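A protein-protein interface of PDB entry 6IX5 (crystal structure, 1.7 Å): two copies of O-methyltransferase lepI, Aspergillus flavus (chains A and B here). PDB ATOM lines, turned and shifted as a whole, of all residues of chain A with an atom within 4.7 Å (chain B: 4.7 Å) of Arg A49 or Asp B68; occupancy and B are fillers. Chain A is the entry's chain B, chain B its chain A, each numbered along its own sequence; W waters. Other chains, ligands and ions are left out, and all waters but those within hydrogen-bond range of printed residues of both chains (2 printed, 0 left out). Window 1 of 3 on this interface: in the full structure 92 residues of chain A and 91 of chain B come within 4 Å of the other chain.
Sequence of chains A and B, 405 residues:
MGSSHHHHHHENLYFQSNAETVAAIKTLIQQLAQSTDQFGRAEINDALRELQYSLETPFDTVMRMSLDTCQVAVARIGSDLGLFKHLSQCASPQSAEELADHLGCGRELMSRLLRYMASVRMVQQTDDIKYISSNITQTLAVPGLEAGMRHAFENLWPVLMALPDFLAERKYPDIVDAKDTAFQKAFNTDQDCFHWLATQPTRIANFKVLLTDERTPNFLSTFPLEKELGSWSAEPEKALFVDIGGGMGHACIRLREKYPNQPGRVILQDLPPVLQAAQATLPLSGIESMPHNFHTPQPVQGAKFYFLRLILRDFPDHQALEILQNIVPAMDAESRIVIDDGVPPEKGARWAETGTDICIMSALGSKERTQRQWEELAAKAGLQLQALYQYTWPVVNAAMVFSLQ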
ATOM      1  N   ASN A  45       0.299  19.338 -13.446  1.00  0.00           N
ATOM      2  CA  ASN A  45       0.667  20.758 -13.319  1.00  0.00           C
ATOM      3  C   ASN A  45       1.321  21.292 -14.587  1.00  0.00           C
ATOM      4  O   ASN A  45       1.014  22.403 -15.019  1.00  0.00           O
ATOM      5  CB  ASN A  45       1.591  20.971 -12.122  1.00  0.00           C
ATOM      6  CG  ASN A  45       0.834  21.356 -10.889  1.00  0.00           C
ATOM      7  OD1 ASN A  45       1.422  21.638  -9.848  1.00  0.00           O
ATOM      8  ND2 ASN A  45      -0.488  21.374 -10.988  1.00  0.00           N
ATOM      9  N   ASP A  46       2.237  20.534 -15.185  1.00  0.00           N
ATOM     10  CA  ASP A  46       2.862  20.998 -16.424  1.00  0.00           C
ATOM     11  C   ASP A  46       1.818  21.147 -17.529  1.00  0.00           C
ATOM     12  O   ASP A  46       1.878  22.083 -18.346  1.00  0.00           O
ATOM     13  CB  ASP A  46       3.976  20.037 -16.857  1.00  0.00           C
ATOM     14  CG  ASP A  46       5.236  20.191 -16.006  1.00  0.00           C
ATOM     15  OD1 ASP A  46       5.264  21.100 -15.126  1.00  0.00           O
ATOM     16  OD2 ASP A  46       6.195  19.398 -16.199  1.00  0.00           O
ATOM     17  N   ALA A  47       0.827  20.258 -17.544  1.00  0.00           N
ATOM     18  CA  ALA A  47      -0.226  20.362 -18.556  1.00  0.00           C
ATOM     19  C   ALA A  47      -1.108  21.574 -18.304  1.00  0.00           C
ATOM     20  O   ALA A  47      -1.572  22.227 -19.258  1.00  0.00           O
ATOM     21  CB  ALA A  47      -1.076  19.081 -18.578  1.00  0.00           C
ATOM     22  N   LEU A  48      -1.379  21.888 -17.030  1.00  0.00           N
ATOM     23  CA  LEU A  48      -2.156  23.097 -16.756  1.00  0.00           C
ATOM     24  C   LEU A  48      -1.404  24.337 -17.234  1.00  0.00           C
ATOM     25  O   LEU A  48      -2.008  25.274 -17.760  1.00  0.00           O
ATOM     26  CB  LEU A  48      -2.473  23.220 -15.286  1.00  0.00           C
ATOM     27  CG  LEU A  48      -3.321  22.068 -14.701  1.00  0.00           C
ATOM     28  CD1 LEU A  48      -3.461  22.187 -13.175  1.00  0.00           C
ATOM     29  CD2 LEU A  48      -4.737  22.017 -15.335  1.00  0.00           C
ATOM     30  N   ARG A  49      -0.084  24.377 -17.014  1.00  0.00           N
ATOM     31  CA  ARG A  49       0.692  25.510 -17.527  1.00  0.00           C
ATOM     32  C   ARG A  49       0.569  25.602 -19.038  1.00  0.00           C
ATOM     33  O   ARG A  49       0.379  26.692 -19.605  1.00  0.00           O
ATOM     34  CB  ARG A  49       2.182  25.374 -17.176  1.00  0.00           C
ATOM     35  CG  ARG A  49       2.515  25.477 -15.761  1.00  0.00           C
ATOM     36  CD  ARG A  49       4.056  25.537 -15.573  1.00  0.00           C
ATOM     37  NE  ARG A  49       4.461  25.717 -14.168  1.00  0.00           N
ATOM     38  CZ  ARG A  49       5.301  26.665 -13.754  1.00  0.00           C
ATOM     39  NH1 ARG A  49       5.598  26.765 -12.454  1.00  0.00           N
ATOM     40  NH2 ARG A  49       5.867  27.484 -14.635  1.00  0.00           N
ATOM     41  N   GLU A  50       0.749  24.464 -19.712  1.00  0.00           N
ATOM     42  CA  GLU A  50       0.710  24.469 -21.171  1.00  0.00           C
ATOM     43  C   GLU A  50      -0.651  24.946 -21.666  1.00  0.00           C
ATOM     44  O   GLU A  50      -0.744  25.724 -22.638  1.00  0.00           O
ATOM     45  CB  GLU A  50       1.016  23.073 -21.705  1.00  0.00           C
ATOM     46  CG  GLU A  50       1.221  23.056 -23.204  1.00  0.00           C
ATOM     47  CD  GLU A  50       1.434  21.642 -23.726  1.00  0.00           C
ATOM     48  OE1 GLU A  50       0.449  21.032 -24.228  1.00  0.00           O
ATOM     49  OE2 GLU A  50       2.572  21.126 -23.587  1.00  0.00           O
ATOM     50  N   LEU A  51      -1.717  24.476 -21.020  1.00  0.00           N
ATOM     51  CA  LEU A  51      -3.066  24.938 -21.372  1.00  0.00           C
ATOM     52  C   LEU A  51      -3.201  26.442 -21.197  1.00  0.00           C
ATOM     53  O   LEU A  51      -3.723  27.133 -22.080  1.00  0.00           O
ATOM     54  CB  LEU A  51      -4.119  24.237 -20.524  1.00  0.00           C
ATOM     55  CG  LEU A  51      -4.469  22.842 -21.000  1.00  0.00           C
ATOM     56  CD1 LEU A  51      -5.188  22.116 -19.840  1.00  0.00           C
ATOM     57  CD2 LEU A  51      -5.306  22.855 -22.280  1.00  0.00           C
ATOM     58  N   GLN A  52      -2.735  26.955 -20.060  1.00  0.00           N
ATOM     59  CA  GLN A  52      -2.802  28.380 -19.790  1.00  0.00           C
ATOM     60  C   GLN A  52      -2.107  29.190 -20.885  1.00  0.00           C
ATOM     61  O   GLN A  52      -2.644  30.203 -21.351  1.00  0.00           O
ATOM     62  CB  GLN A  52      -2.168  28.636 -18.427  1.00  0.00           C
ATOM     63  CG  GLN A  52      -2.160  30.038 -17.969  1.00  0.00           C
ATOM     64  CD  GLN A  52      -1.106  30.272 -16.895  1.00  0.00           C
ATOM     65  OE1 GLN A  52      -0.832  29.388 -16.082  1.00  0.00           O
ATOM     66  NE2 GLN A  52      -0.486  31.453 -16.912  1.00  0.00           N
ATOM     67  N   TYR A  53      -0.916  28.743 -21.318  1.00  0.00           N
ATOM     68  CA  TYR A  53      -0.150  29.478 -22.317  1.00  0.00           C
ATOM     69  C   TYR A  53      -0.818  29.405 -23.681  1.00  0.00           C
ATOM     70  O   TYR A  53      -0.762  30.365 -24.435  1.00  0.00           O
ATOM     71  CB  TYR A  53       1.294  28.950 -22.437  1.00  0.00           C
ATOM     72  CG  TYR A  53       2.142  29.190 -21.203  1.00  0.00           C
ATOM     73  CD1 TYR A  53       1.653  29.884 -20.092  1.00  0.00           C
ATOM     74  CD2 TYR A  53       3.410  28.677 -21.125  1.00  0.00           C
ATOM     75  CE1 TYR A  53       2.436  30.076 -18.947  1.00  0.00           C
ATOM     76  CE2 TYR A  53       4.194  28.853 -20.014  1.00  0.00           C
ATOM     77  CZ  TYR A  53       3.714  29.553 -18.921  1.00  0.00           C
ATOM     78  OH  TYR A  53       4.538  29.698 -17.838  1.00  0.00           O
ATOM     79  N   TRP A 351      10.395  23.041 -18.204  1.00  0.00           N
ATOM     80  CA  TRP A 351      10.865  24.364 -17.785  1.00  0.00           C
ATOM     81  C   TRP A 351      11.801  24.327 -16.583  1.00  0.00           C
ATOM     82  O   TRP A 351      12.672  25.194 -16.464  1.00  0.00           O
ATOM     83  CB  TRP A 351       9.679  25.285 -17.510  1.00  0.00           C
ATOM     84  CG  TRP A 351       8.775  24.842 -16.404  1.00  0.00           C
ATOM     85  CD1 TRP A 351       7.681  24.008 -16.501  1.00  0.00           C
ATOM     86  CD2 TRP A 351       8.926  25.155 -15.016  1.00  0.00           C
ATOM     87  NE1 TRP A 351       7.139  23.816 -15.245  1.00  0.00           N
ATOM     88  CE2 TRP A 351       7.891  24.517 -14.328  1.00  0.00           C
ATOM     89  CE3 TRP A 351       9.850  25.940 -14.281  1.00  0.00           C
ATOM     90  CZ2 TRP A 351       7.737  24.640 -12.930  1.00  0.00           C
ATOM     91  CZ3 TRP A 351       9.698  26.057 -12.922  1.00  0.00           C
ATOM     92  CH2 TRP A 351       8.640  25.410 -12.254  1.00  0.00           C
ATOM     93  N   GLN B  52      -2.899  25.157 -10.465  1.00  0.00           N
ATOM     94  CA  GLN B  52      -1.467  24.903 -10.469  1.00  0.00           C
ATOM     95  C   GLN B  52      -0.846  25.243  -9.114  1.00  0.00           C
ATOM     96  O   GLN B  52      -0.064  24.446  -8.555  1.00  0.00           O
ATOM     97  CB  GLN B  52      -0.834  25.717 -11.588  1.00  0.00           C
ATOM     98  CG  GLN B  52       0.620  25.503 -11.788  1.00  0.00           C
ATOM     99  CD  GLN B  52       1.242  26.709 -12.433  1.00  0.00           C
ATOM    100  OE1 GLN B  52       2.387  27.075 -12.128  1.00  0.00           O
ATOM    101  NE2 GLN B  52       0.483  27.367 -13.302  1.00  0.00           N
ATOM    102  N   MET B  63      10.590  26.716  -6.768  1.00  0.00           N
ATOM    103  CA  MET B  63      11.154  26.586  -8.110  1.00  0.00           C
ATOM    104  C   MET B  63      10.492  27.536  -9.262  1.00  0.00           C
ATOM    105  O   MET B  63      11.066  28.211 -10.105  1.00  0.00           O
ATOM    106  CB  MET B  63      11.149  25.145  -8.637  1.00  0.00           C
ATOM    107  CG  MET B  63      12.193  24.301  -7.996  1.00  0.00           C
ATOM    108  SD  MET B  63      13.838  24.843  -8.508  1.00  0.00           S
ATOM    109  CE  MET B  63      13.740  24.531 -10.256  1.00  0.00           C
ATOM    110  N   ARG B  64       9.135  27.551  -9.120  1.00  0.00           N
ATOM    111  CA  ARG B  64       8.349  28.378 -10.032  1.00  0.00           C
ATOM    112  C   ARG B  64       8.683  29.848  -9.830  1.00  0.00           C
ATOM    113  O   ARG B  64       8.925  30.595 -10.798  1.00  0.00           O
ATOM    114  CB  ARG B  64       6.836  28.129  -9.755  1.00  0.00           C
ATOM    115  CG  ARG B  64       5.930  29.209 -10.305  1.00  0.00           C
ATOM    116  CD  ARG B  64       4.477  28.808 -10.089  1.00  0.00           C
ATOM    117  NE  ARG B  64       4.057  28.892  -8.700  1.00  0.00           N
ATOM    118  CZ  ARG B  64       3.838  30.008  -8.004  1.00  0.00           C
ATOM    119  NH1 ARG B  64       4.080  31.243  -8.514  1.00  0.00           N
ATOM    120  NH2 ARG B  64       3.402  29.868  -6.753  1.00  0.00           N
ATOM    121  N   MET B  65       8.724  30.291  -8.561  1.00  0.00           N
ATOM    122  CA  MET B  65       9.039  31.703  -8.323  1.00  0.00           C
ATOM    123  C   MET B  65      10.453  32.024  -8.775  1.00  0.00           C
ATOM    124  O   MET B  65      10.718  33.131  -9.279  1.00  0.00           O
ATOM    125  CB  MET B  65       8.877  32.039  -6.844  1.00  0.00           C
ATOM    126  CG  MET B  65       7.437  32.066  -6.408  1.00  0.00           C
ATOM    127  SD  MET B  65       7.386  32.439  -4.628  1.00  0.00           S
ATOM    128  CE  MET B  65       5.607  32.373  -4.384  1.00  0.00           C
ATOM    129  N   SER B  66      11.370  31.073  -8.607  1.00  0.00           N
ATOM    130  CA  SER B  66      12.766  31.331  -8.959  1.00  0.00           C
ATOM    131  C   SER B  66      12.954  31.397 -10.466  1.00  0.00           C
ATOM    132  O   SER B  66      13.810  32.146 -10.967  1.00  0.00           O
ATOM    133  CB  SER B  66      13.670  30.218  -8.429  1.00  0.00           C
ATOM    134  OG  SER B  66      13.709  30.129  -6.997  1.00  0.00           O
ATOM    135  N   LEU B  67      12.231  30.578 -11.200  1.00  0.00           N
ATOM    136  CA  LEU B  67      12.534  30.426 -12.625  1.00  0.00           C
ATOM    137  C   LEU B  67      11.565  31.175 -13.542  1.00  0.00           C
ATOM    138  O   LEU B  67      11.892  31.378 -14.714  1.00  0.00           O
ATOM    139  CB  LEU B  67      12.547  28.946 -13.010  1.00  0.00           C
ATOM    140  CG  LEU B  67      13.676  28.132 -12.369  1.00  0.00           C
ATOM    141  CD1 LEU B  67      13.563  26.649 -12.828  1.00  0.00           C
ATOM    142  CD2 LEU B  67      15.066  28.705 -12.741  1.00  0.00           C
ATOM    143  N   ASP B  68      10.393  31.599 -13.070  1.00  0.00           N
ATOM    144  CA  ASP B  68       9.478  32.162 -14.076  1.00  0.00           C
ATOM    145  C   ASP B  68      10.015  33.518 -14.574  1.00  0.00           C
ATOM    146  O   ASP B  68       9.723  33.933 -15.709  1.00  0.00           O
ATOM    147  CB  ASP B  68       8.026  32.217 -13.525  1.00  0.00           C
ATOM    148  CG  ASP B  68       7.223  30.824 -13.646  1.00  0.00           C
ATOM    149  OD1 ASP B  68       7.737  29.729 -14.078  1.00  0.00           O
ATOM    150  OD2 ASP B  68       6.015  30.838 -13.288  1.00  0.00           O
ATOM    151  N   THR B  69      10.858  34.166 -13.781  1.00  0.00           N
ATOM    152  CA  THR B  69      11.757  35.286 -14.111  1.00  0.00           C
ATOM    153  C   THR B  69      12.513  35.150 -15.449  1.00  0.00           C
ATOM    154  O   THR B  69      12.772  36.129 -16.178  1.00  0.00           O
ATOM    155  CB  THR B  69      12.801  35.361 -12.977  1.00  0.00           C
ATOM    156  OG1 THR B  69      12.194  35.489 -11.689  1.00  0.00           O
ATOM    157  CG2 THR B  69      13.753  36.402 -13.179  1.00  0.00           C
ATOM    158  N   CYS B  70      12.908  33.924 -15.756  1.00  0.00           N
ATOM    159  CA  CYS B  70      13.667  33.665 -16.975  1.00  0.00           C
ATOM    160  C   CYS B  70      12.917  34.096 -18.223  1.00  0.00           C
ATOM    161  O   CYS B  70      13.533  34.341 -19.263  1.00  0.00           O
ATOM    162  CB  CYS B  70      13.945  32.176 -17.121  1.00  0.00           C
ATOM    163  SG  CYS B  70      15.138  31.584 -15.922  1.00  0.00           S
ATOM    164  N   GLN B  71      11.593  34.121 -18.174  1.00  0.00           N
ATOM    165  CA  GLN B  71      10.856  34.283 -19.422  1.00  0.00           C
ATOM    166  C   GLN B  71      11.083  35.673 -19.990  1.00  0.00           C
ATOM    167  O   GLN B  71      11.296  35.824 -21.194  1.00  0.00           O
ATOM    168  CB  GLN B  71       9.356  34.025 -19.213  1.00  0.00           C
ATOM    169  CG  GLN B  71       9.067  32.585 -18.849  1.00  0.00           C
ATOM    170  CD  GLN B  71       7.638  32.185 -19.102  1.00  0.00           C
ATOM    171  OE1 GLN B  71       7.015  32.684 -20.025  1.00  0.00           O
ATOM    172  NE2 GLN B  71       7.115  31.247 -18.300  1.00  0.00           N
ATOM    173  N   VAL B  72      11.026  36.722 -19.155  1.00  0.00           N
ATOM    174  CA  VAL B  72      11.193  38.070 -19.693  1.00  0.00           C
ATOM    175  C   VAL B  72      12.611  38.283 -20.189  1.00  0.00           C
ATOM    176  O   VAL B  72      12.833  38.955 -21.208  1.00  0.00           O
ATOM    177  CB  VAL B  72      10.823  39.128 -18.645  1.00  0.00           C
ATOM    178  CG1 VAL B  72      11.062  40.511 -19.226  1.00  0.00           C
ATOM    179  CG2 VAL B  72       9.408  38.984 -18.286  1.00  0.00           C
HETATM  180  O   HOH W   1       1.102  29.492 -14.492  1.00  0.00           O
HETATM  181  O   HOH W   2       3.741  29.511 -13.367  1.00  0.00           O
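Of the printed residues of chain B, Arg A49 touches Gln B52 (3.2 Å), Arg B64 (3.3 Å) and Asp B68 (3.0 Å). Of chain A, only Arg A49 (3.0 Å) comes within 4 Å of Asp B68. Printed residues of chain B within 4 Å of Trp A351: Met B63 (3.8 Å), Arg B64 (3.7 Å) and Leu B67 (3.9 Å). Printed residues of chain A within 4 Å of Arg B64: Arg A49 (3.3 Å) and Trp A351 (3.7 Å). Ser B66 touches none of the printed residues of chain A. Glu A50 touches none of the printed residues of chain B. The nearest printed residue of chain B that does not touch Asn A45 is Arg B64 (7.8 Å).
Of the 10 printed residues of chain A, 5 touch a printed residue of chain B. Along chain A the printed residues that touch a printed residue of chain B span positions 45 to 351. Printed residues of chain B that touch a printed residue of chain A: Gln B52, Met B63, Arg B64, Leu B67, Asp B68 and Gln B71. Hydrophobic or aromatic side chains of chain B within 4 Å of the printed part of chain A: Leu B67. Among the printed residues, 9 pairs touch across the chains. Among the printed residues, Asp or Glu carboxylates within 4 Å of a Lys or Arg side-chain nitrogen of the other chain: Arg A49 with Asp B68 (3.0 Å).
Gln A52 touches its own counterpart, Gln B52. Position printed for both chains: 52.
The side-chain amide oxygen of Asn A45 sits close to the backbone carbonyl oxygen of Gln B52, at 3.4 Å. OE1 of Gln B52 sits at hydrogen-bond distance from NE of Arg A49, at 3.2 Å. The side-chain carboxylate (OD1) of Asp B68 is in salt-bridge range of the guanidinium group (NH2) of Arg A49, at 3.0 Å. OH of Tyr A53 sits at hydrogen-bond distance from NE2 of Gln B71 (3.0 Å).
Among the printed residues, pairs that only touch across the chains: Arg A49 with Arg B64, Gln A52 with Gln B52, Trp A351 with Met B63, Trp A351 with Arg B64 and Trp A351 with Leu B67.
Water W1 bridges the side-chain amide oxygen of Gln A52 and the side-chain amide nitrogen of Gln B52. Water W2 lies within hydrogen-bond range of OD2 of Asp B68, OE1 of Gln B52 and NH2 of Arg A49.
The backbone carbonyl oxygen (O) of Leu B67 lies close to the side-chain sulfur (SG) of Cys B70, at 3.5 Å. The side-chain carboxylate (OD1) of Asp A46 sits at hydrogen-bond distance from the indole nitrogen (NE1) of Trp A351 (3.3 Å).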
